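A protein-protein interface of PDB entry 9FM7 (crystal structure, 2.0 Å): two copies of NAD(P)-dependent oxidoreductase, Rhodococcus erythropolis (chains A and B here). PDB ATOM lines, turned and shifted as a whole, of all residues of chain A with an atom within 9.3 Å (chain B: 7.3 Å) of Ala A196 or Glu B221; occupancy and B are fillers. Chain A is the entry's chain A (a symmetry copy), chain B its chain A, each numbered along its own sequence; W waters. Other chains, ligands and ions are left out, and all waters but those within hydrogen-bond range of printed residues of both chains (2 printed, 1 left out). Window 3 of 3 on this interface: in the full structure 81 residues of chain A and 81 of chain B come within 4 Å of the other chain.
Water W1 bridges the side-chain carboxylate (OE2) of Glu A197 (2.7 Å) and the guanidinium group (NH2) of Arg B153 (3.1 Å).
Water W2 lies within hydrogen-bond range of OE2 of Glu B221, N of Ala A196 and N of Ile A195.
No position is printed for both chains.
Of the 11 pairs that touch across the chains among the printed residues, none has its exchanged pair printed and touching as well.
CD1 of Leu B217 touches CZ of Phe A181 (3.6 Å).
CE2 of Phe B220 touches CB of Ala A185 (3.5 Å).
Ile B165 touches Val A193.
CD1 of Leu B217 touches CG2 of Ile A195, at 3.5 Å.
Ala A196 touches Glu B221.
Glu A197 touches Ile B165.
Arg A199 touches Leu B217.
NE2 of His A200 touches CB of Arg B153, at 3.5 Å.
Leu A202 touches Leu B217.
The backbone NH of Val A193 sits at hydrogen-bond distance from the backbone carbonyl oxygen of Val A188 (3.1 Å).
A ring nitrogen (ND1) of His A200 sits close to the backbone carbonyl oxygen (O) of Glu A197, 3.5 Å away.
A ring nitrogen (NE2) of His A200 is in hydrogen-bond range of the side-chain hydroxyl of Ser A201 (3.4 Å).
Of the 14 printed residues of chain A, 9 touch a printed residue of chain B.
Hydrophobic or aromatic side chains of chain A within 4 Å of the printed part of chain B: Phe A181, Ala A185, Val A193, Ile A195, Ala A196, His A200 and Leu A202.
Of the 13 printed residues of chain B, 5 touch a printed residue of chain A.
Printed residues of chain B that touch a printed residue of chain A: Arg B153, Ile B165, Leu B217, Phe B220 and Glu B221.
Among the printed residues, 11 pairs touch across the chains.
Among the printed residues, Asp or Glu carboxylates within 4 Å of a Lys or Arg side-chain nitrogen of the other chain: Glu A197 with Arg B153 and Arg A199 with Glu B221.
Of the printed residues of chain B, Phe A181 touches Leu B217.
Printed residues of chain B within 4 Å of Val A193: Ile B165 (3.9 Å).
Of the printed residues of chain B, Ala A196 touches Glu B221.
Of the printed residues of chain A, Phe B220 touches Ala A185.
No residue of chain A comes within 4 Å of Ser B222.
The nearest residue of chain A that does not touch Glu B221 is Ile A195 (4.5 Å).
OE1 of Glu A197 is in salt-bridge range of NE of Arg B153, 2.9 Å away.
The guanidinium group of Arg A199 lies within salt-bridge range of the side-chain carboxylate of Glu B221, 3.2 Å away.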
ATOM      1  N   PHE A 181      11.691  22.533  10.516  1.00  0.00           N
ATOM      2  CA  PHE A 181      10.544  22.694  11.397  1.00  0.00           C
ATOM      3  C   PHE A 181      10.527  21.607  12.478  1.00  0.00           C
ATOM      4  O   PHE A 181      10.096  21.881  13.594  1.00  0.00           O
ATOM      5  CB  PHE A 181       9.210  22.705  10.635  1.00  0.00           C
ATOM      6  CG  PHE A 181       8.011  23.007  11.538  1.00  0.00           C
ATOM      7  CD1 PHE A 181       7.803  24.279  12.045  1.00  0.00           C
ATOM      8  CD2 PHE A 181       7.100  22.016  11.875  1.00  0.00           C
ATOM      9  CE1 PHE A 181       6.723  24.553  12.872  1.00  0.00           C
ATOM     10  CE2 PHE A 181       6.032  22.287  12.727  1.00  0.00           C
ATOM     11  CZ  PHE A 181       5.829  23.551  13.199  1.00  0.00           C
ATOM     12  N   ALA A 185      10.462  22.563  16.478  1.00  0.00           N
ATOM     13  CA  ALA A 185       9.469  22.106  17.442  1.00  0.00           C
ATOM     14  C   ALA A 185      10.108  21.256  18.549  1.00  0.00           C
ATOM     15  O   ALA A 185       9.698  21.320  19.712  1.00  0.00           O
ATOM     16  CB  ALA A 185       8.387  21.315  16.727  1.00  0.00           C
ATOM     17  N   VAL A 188      11.508  23.752  20.950  1.00  0.00           N
ATOM     18  CA  VAL A 188      10.493  24.327  21.813  1.00  0.00           C
ATOM     19  C   VAL A 188      10.145  23.335  22.924  1.00  0.00           C
ATOM     20  O   VAL A 188      10.007  23.713  24.088  1.00  0.00           O
ATOM     21  CB  VAL A 188       9.256  24.718  20.982  1.00  0.00           C
ATOM     22  CG1 VAL A 188       8.045  25.060  21.855  1.00  0.00           C
ATOM     23  CG2 VAL A 188       9.574  25.874  20.030  1.00  0.00           C
ATOM     24  N   ARG A 189       9.961  22.066  22.560  1.00  0.00           N
ATOM     25  CA  ARG A 189       9.536  21.074  23.532  1.00  0.00           C
ATOM     26  C   ARG A 189      10.633  20.873  24.572  1.00  0.00           C
ATOM     27  O   ARG A 189      10.330  20.783  25.750  1.00  0.00           O
ATOM     28  CB  ARG A 189       9.115  19.799  22.805  1.00  0.00           C
ATOM     29  CG  ARG A 189       8.374  18.811  23.687  1.00  0.00           C
ATOM     30  CD  ARG A 189       7.910  17.615  22.860  1.00  0.00           C
ATOM     31  NE  ARG A 189       9.061  16.873  22.323  1.00  0.00           N
ATOM     32  CZ  ARG A 189       9.018  15.932  21.378  1.00  0.00           C
ATOM     33  NH1 ARG A 189       7.858  15.564  20.856  1.00  0.00           N
ATOM     34  NH2 ARG A 189      10.138  15.366  20.965  1.00  0.00           N
ATOM     35  N   VAL A 193       8.286  24.380  26.638  1.00  0.00           N
ATOM     36  CA  VAL A 193       7.275  25.304  26.151  1.00  0.00           C
ATOM     37  C   VAL A 193       6.293  24.508  25.300  1.00  0.00           C
ATOM     38  O   VAL A 193       6.700  23.544  24.661  1.00  0.00           O
ATOM     39  CB  VAL A 193       7.982  26.436  25.379  1.00  0.00           C
ATOM     40  CG1 VAL A 193       7.016  27.313  24.592  1.00  0.00           C
ATOM     41  CG2 VAL A 193       8.810  27.315  26.301  1.00  0.00           C
ATOM     42  N   ALA A 194       5.014  24.916  25.275  1.00  0.00           N
ATOM     43  CA  ALA A 194       3.987  24.188  24.543  1.00  0.00           C
ATOM     44  C   ALA A 194       4.186  24.303  23.025  1.00  0.00           C
ATOM     45  O   ALA A 194       4.146  25.381  22.463  1.00  0.00           O
ATOM     46  CB  ALA A 194       2.621  24.704  24.928  1.00  0.00           C
ATOM     47  N   ILE A 195       4.339  23.172  22.349  1.00  0.00           N
ATOM     48  CA  ILE A 195       4.518  23.182  20.908  1.00  0.00           C
ATOM     49  C   ILE A 195       3.289  23.818  20.248  1.00  0.00           C
ATOM     50  O   ILE A 195       3.402  24.415  19.195  1.00  0.00           O
ATOM     51  CB  ILE A 195       4.821  21.750  20.439  1.00  0.00           C
ATOM     52  CG1 ILE A 195       6.321  21.546  20.283  1.00  0.00           C
ATOM     53  CG2 ILE A 195       4.063  21.378  19.167  1.00  0.00           C
ATOM     54  CD1 ILE A 195       6.691  20.135  19.873  1.00  0.00           C
ATOM     55  N   ALA A 196       2.116  23.688  20.883  1.00  0.00           N
ATOM     56  CA  ALA A 196       0.874  24.271  20.404  1.00  0.00           C
ATOM     57  C   ALA A 196       0.999  25.772  20.147  1.00  0.00           C
ATOM     58  O   ALA A 196       0.277  26.308  19.316  1.00  0.00           O
ATOM     59  CB  ALA A 196      -0.236  24.013  21.412  1.00  0.00           C
ATOM     60  N   GLU A 197       1.865  26.461  20.891  1.00  0.00           N
ATOM     61  CA  GLU A 197       1.925  27.909  20.788  1.00  0.00           C
ATOM     62  C   GLU A 197       2.743  28.334  19.561  1.00  0.00           C
ATOM     63  O   GLU A 197       2.931  29.536  19.329  1.00  0.00           O
ATOM     64  CB  GLU A 197       2.410  28.491  22.122  1.00  0.00           C
ATOM     65  CG  GLU A 197       1.435  28.265  23.284  1.00  0.00           C
ATOM     66  CD  GLU A 197       0.132  29.027  23.123  1.00  0.00           C
ATOM     67  OE1 GLU A 197       0.103  30.013  22.364  1.00  0.00           O
ATOM     68  OE2 GLU A 197      -0.879  28.632  23.713  1.00  0.00           O
ATOM     69  N   MET A 198       3.202  27.366  18.754  1.00  0.00           N
ATOM     70  CA  MET A 198       3.759  27.658  17.442  1.00  0.00           C
ATOM     71  C   MET A 198       2.636  27.820  16.410  1.00  0.00           C
ATOM     72  O   MET A 198       2.842  28.453  15.367  1.00  0.00           O
ATOM     73  CB  MET A 198       4.709  26.545  16.989  1.00  0.00           C
ATOM     74  CG  MET A 198       5.915  26.311  17.894  1.00  0.00           C
ATOM     75  SD  MET A 198       6.729  24.723  17.583  1.00  0.00           S
ATOM     76  CE  MET A 198       7.969  25.111  16.339  1.00  0.00           C
ATOM     77  N   ARG A 199       1.457  27.220  16.676  1.00  0.00           N
ATOM     78  CA  ARG A 199       0.503  26.907  15.615  1.00  0.00           C
ATOM     79  C   ARG A 199      -0.043  28.178  14.970  1.00  0.00           C
ATOM     80  O   ARG A 199      -0.149  28.283  13.737  1.00  0.00           O
ATOM     81  CB  ARG A 199      -0.633  26.033  16.172  1.00  0.00           C
ATOM     82  CG  ARG A 199      -1.687  25.624  15.149  1.00  0.00           C
ATOM     83  CD  ARG A 199      -2.523  24.456  15.672  1.00  0.00           C
ATOM     84  NE  ARG A 199      -2.981  24.793  17.029  1.00  0.00           N
ATOM     85  CZ  ARG A 199      -2.982  23.984  18.064  1.00  0.00           C
ATOM     86  NH1 ARG A 199      -2.727  22.700  17.902  1.00  0.00           N
ATOM     87  NH2 ARG A 199      -3.322  24.447  19.255  1.00  0.00           N
ATOM     88  N   HIS A 200      -0.370  29.170  15.808  1.00  0.00           N
ATOM     89  CA  HIS A 200      -1.114  30.329  15.362  1.00  0.00           C
ATOM     90  C   HIS A 200      -0.248  31.237  14.491  1.00  0.00           C
ATOM     91  O   HIS A 200      -0.807  32.025  13.728  1.00  0.00           O
ATOM     92  CB  HIS A 200      -1.709  31.130  16.522  1.00  0.00           C
ATOM     93  CG  HIS A 200      -0.669  31.736  17.401  1.00  0.00           C
ATOM     94  ND1 HIS A 200      -0.071  31.017  18.412  1.00  0.00           N
ATOM     95  CD2 HIS A 200      -0.086  32.957  17.401  1.00  0.00           C
ATOM     96  CE1 HIS A 200       0.837  31.792  19.003  1.00  0.00           C
ATOM     97  NE2 HIS A 200       0.853  32.967  18.397  1.00  0.00           N
ATOM     98  N   SER A 201       1.088  31.065  14.557  1.00  0.00           N
ATOM     99  CA  SER A 201       2.022  31.877  13.786  1.00  0.00           C
ATOM    100  C   SER A 201       2.378  31.268  12.430  1.00  0.00           C
ATOM    101  O   SER A 201       3.034  31.941  11.623  1.00  0.00           O
ATOM    102  CB  SER A 201       3.301  32.094  14.571  1.00  0.00           C
ATOM    103  OG  SER A 201       2.989  32.767  15.775  1.00  0.00           O
ATOM    104  N   LEU A 202       2.069  29.980  12.233  1.00  0.00           N
ATOM    105  CA  LEU A 202       2.576  29.259  11.076  1.00  0.00           C
ATOM    106  C   LEU A 202       2.342  30.050   9.787  1.00  0.00           C
ATOM    107  O   LEU A 202       3.242  30.238   8.966  1.00  0.00           O
ATOM    108  CB  LEU A 202       1.939  27.871  11.032  1.00  0.00           C
ATOM    109  CG  LEU A 202       2.749  26.682  11.558  1.00  0.00           C
ATOM    110  CD1 LEU A 202       3.885  26.985  12.480  1.00  0.00           C
ATOM    111  CD2 LEU A 202       1.845  25.672  12.195  1.00  0.00           C
ATOM    112  N   ARG B 153      -0.699  37.288  21.054  1.00  0.00           N
ATOM    113  CA  ARG B 153      -1.011  36.069  21.775  1.00  0.00           C
ATOM    114  C   ARG B 153      -0.120  35.927  23.001  1.00  0.00           C
ATOM    115  O   ARG B 153       1.107  36.088  22.914  1.00  0.00           O
ATOM    116  CB  ARG B 153      -0.717  34.841  20.915  1.00  0.00           C
ATOM    117  CG  ARG B 153      -0.884  33.518  21.649  1.00  0.00           C
ATOM    118  CD  ARG B 153      -2.143  32.810  21.237  1.00  0.00           C
ATOM    119  NE  ARG B 153      -2.279  31.521  21.917  1.00  0.00           N
ATOM    120  CZ  ARG B 153      -3.366  31.161  22.573  1.00  0.00           C
ATOM    121  NH1 ARG B 153      -4.453  31.903  22.489  1.00  0.00           N
ATOM    122  NH2 ARG B 153      -3.344  30.075  23.313  1.00  0.00           N
ATOM    123  N   ILE B 165      10.005  30.440  21.412  1.00  0.00           N
ATOM    124  CA  ILE B 165       9.260  30.283  20.162  1.00  0.00           C
ATOM    125  C   ILE B 165       9.862  31.154  19.056  1.00  0.00           C
ATOM    126  O   ILE B 165       9.889  30.733  17.895  1.00  0.00           O
ATOM    127  CB  ILE B 165       7.758  30.540  20.402  1.00  0.00           C
ATOM    128  CG1 ILE B 165       7.181  29.439  21.272  1.00  0.00           C
ATOM    129  CG2 ILE B 165       6.954  30.703  19.105  1.00  0.00           C
ATOM    130  CD1 ILE B 165       5.807  29.788  21.813  1.00  0.00           C
ATOM    131  N   GLU B 215       0.218  19.763   9.871  1.00  0.00           N
ATOM    132  CA  GLU B 215       0.037  18.335  10.007  1.00  0.00           C
ATOM    133  C   GLU B 215       1.149  17.753  10.893  1.00  0.00           C
ATOM    134  O   GLU B 215       0.912  16.841  11.703  1.00  0.00           O
ATOM    135  CB  GLU B 215      -0.101  17.837   8.561  1.00  0.00           C
ATOM    136  CG  GLU B 215      -0.168  16.323   8.416  1.00  0.00           C
ATOM    137  CD  GLU B 215      -0.256  15.837   6.974  1.00  0.00           C
ATOM    138  OE1 GLU B 215      -0.544  16.683   6.110  1.00  0.00           O
ATOM    139  OE2 GLU B 215      -0.013  14.634   6.707  1.00  0.00           O
ATOM    140  N   ALA B 216       2.387  18.256  10.743  1.00  0.00           N
ATOM    141  CA  ALA B 216       3.491  17.818  11.596  1.00  0.00           C
ATOM    142  C   ALA B 216       3.206  18.119  13.073  1.00  0.00           C
ATOM    143  O   ALA B 216       3.547  17.328  13.944  1.00  0.00           O
ATOM    144  CB  ALA B 216       4.767  18.480  11.151  1.00  0.00           C
ATOM    145  N   LEU B 217       2.639  19.295  13.343  1.00  0.00           N
ATOM    146  CA  LEU B 217       2.351  19.740  14.697  1.00  0.00           C
ATOM    147  C   LEU B 217       1.297  18.824  15.319  1.00  0.00           C
ATOM    148  O   LEU B 217       1.451  18.398  16.464  1.00  0.00           O
ATOM    149  CB  LEU B 217       1.873  21.188  14.589  1.00  0.00           C
ATOM    150  CG  LEU B 217       2.289  22.160  15.689  1.00  0.00           C
ATOM    151  CD1 LEU B 217       3.792  22.184  15.771  1.00  0.00           C
ATOM    152  CD2 LEU B 217       1.792  23.560  15.429  1.00  0.00           C
ATOM    153  N   LYS B 218       0.252  18.495  14.536  1.00  0.00           N
ATOM    154  CA  LYS B 218      -0.795  17.573  14.963  1.00  0.00           C
ATOM    155  C   LYS B 218      -0.176  16.236  15.352  1.00  0.00           C
ATOM    156  O   LYS B 218      -0.533  15.646  16.365  1.00  0.00           O
ATOM    157  CB  LYS B 218      -1.823  17.258  13.873  1.00  0.00           C
ATOM    158  CG  LYS B 218      -2.691  18.397  13.346  1.00  0.00           C
ATOM    159  CD  LYS B 218      -3.683  17.882  12.305  1.00  0.00           C
ATOM    160  CE  LYS B 218      -3.960  18.851  11.190  1.00  0.00           C
ATOM    161  NZ  LYS B 218      -4.565  20.084  11.700  1.00  0.00           N
ATOM    162  N   ALA B 219       0.810  15.781  14.570  1.00  0.00           N
ATOM    163  CA  ALA B 219       1.480  14.518  14.833  1.00  0.00           C
ATOM    164  C   ALA B 219       2.418  14.589  16.030  1.00  0.00           C
ATOM    165  O   ALA B 219       2.668  13.559  16.650  1.00  0.00           O
ATOM    166  CB  ALA B 219       2.266  14.077  13.622  1.00  0.00           C
ATOM    167  N   PHE B 220       3.040  15.753  16.263  1.00  0.00           N
ATOM    168  CA  PHE B 220       3.944  15.913  17.389  1.00  0.00           C
ATOM    169  C   PHE B 220       3.097  15.930  18.667  1.00  0.00           C
ATOM    170  O   PHE B 220       3.549  15.442  19.685  1.00  0.00           O
ATOM    171  CB  PHE B 220       4.811  17.179  17.312  1.00  0.00           C
ATOM    172  CG  PHE B 220       5.728  17.376  16.111  1.00  0.00           C
ATOM    173  CD1 PHE B 220       6.228  16.301  15.374  1.00  0.00           C
ATOM    174  CD2 PHE B 220       6.112  18.660  15.739  1.00  0.00           C
ATOM    175  CE1 PHE B 220       7.052  16.511  14.281  1.00  0.00           C
ATOM    176  CE2 PHE B 220       6.920  18.873  14.623  1.00  0.00           C
ATOM    177  CZ  PHE B 220       7.371  17.810  13.889  1.00  0.00           C
ATOM    178  N   GLU B 221       1.866  16.474  18.606  1.00  0.00           N
ATOM    179  CA  GLU B 221       0.989  16.587  19.769  1.00  0.00           C
ATOM    180  C   GLU B 221       0.417  15.216  20.125  1.00  0.00           C
ATOM    181  O   GLU B 221       0.668  14.722  21.223  1.00  0.00           O
ATOM    182  CB  GLU B 221      -0.180  17.559  19.590  1.00  0.00           C
ATOM    183  CG  GLU B 221       0.262  19.005  19.387  1.00  0.00           C
ATOM    184  CD  GLU B 221      -0.501  19.993  20.246  1.00  0.00           C
ATOM    185  OE1 GLU B 221      -1.629  20.400  19.880  1.00  0.00           O
ATOM    186  OE2 GLU B 221       0.046  20.308  21.326  1.00  0.00           O
ATOM    187  N   SER B 222      -0.385  14.632  19.213  1.00  0.00           N
ATOM    188  CA  SER B 222      -0.554  13.186  19.148  1.00  0.00           C
ATOM    189  C   SER B 222       0.832  12.582  19.233  1.00  0.00           C
ATOM    190  O   SER B 222       1.805  13.305  19.140  1.00  0.00           O
ATOM    191  CB  SER B 222      -1.197  12.751  17.859  1.00  0.00           C
ATOM    192  OG  SER B 222      -2.494  13.310  17.740  1.00  0.00           O
ATOM    193  N   GLY B 223       0.936  11.277  19.390  1.00  0.00           N
ATOM    194  CA  GLY B 223       2.207  10.627  19.103  1.00  0.00           C
ATOM    195  C   GLY B 223       2.076   9.769  17.849  1.00  0.00           C
ATOM    196  O   GLY B 223       2.847   8.845  17.649  1.00  0.00           O
ATOM    197  N   GLU B 224       1.095  10.119  17.007  1.00  0.00           N
ATOM    198  CA  GLU B 224       0.579   9.238  15.972  1.00  0.00           C
ATOM    199  C   GLU B 224       1.348   9.500  14.681  1.00  0.00           C
ATOM    200  O   GLU B 224       1.008  10.428  13.946  1.00  0.00           O
ATOM    201  CB  GLU B 224      -0.923   9.493  15.791  1.00  0.00           C
ATOM    202  CG  GLU B 224      -1.813   8.753  16.793  1.00  0.00           C
ATOM    203  CD  GLU B 224      -3.315   8.892  16.578  1.00  0.00           C
ATOM    204  OE1 GLU B 224      -4.034   9.103  17.571  1.00  0.00           O
ATOM    205  OE2 GLU B 224      -3.789   8.790  15.426  1.00  0.00           O
ATOM    206  N   TYR B 225       2.361   8.664  14.426  1.00  0.00           N
ATOM    207  CA  TYR B 225       3.290   8.855  13.328  1.00  0.00           C
ATOM    208  C   TYR B 225       3.065   7.854  12.192  1.00  0.00           C
ATOM    209  O   TYR B 225       3.981   7.664  11.394  1.00  0.00           O
ATOM    210  CB  TYR B 225       4.734   8.660  13.814  1.00  0.00           C
ATOM    211  CG  TYR B 225       5.224   9.645  14.867  1.00  0.00           C
ATOM    212  CD1 TYR B 225       5.008  11.014  14.741  1.00  0.00           C
ATOM    213  CD2 TYR B 225       5.909   9.199  15.990  1.00  0.00           C
ATOM    214  CE1 TYR B 225       5.457  11.903  15.701  1.00  0.00           C
ATOM    215  CE2 TYR B 225       6.362  10.076  16.960  1.00  0.00           C
ATOM    216  CZ  TYR B 225       6.132  11.433  16.815  1.00  0.00           C
ATOM    217  OH  TYR B 225       6.567  12.296  17.776  1.00  0.00           O
HETATM  218  O   HOH W   1      -2.904  26.970  23.027  1.00  0.00           O
HETATM  219  O   HOH W   2       1.769  21.704  22.958  1.00  0.00           O
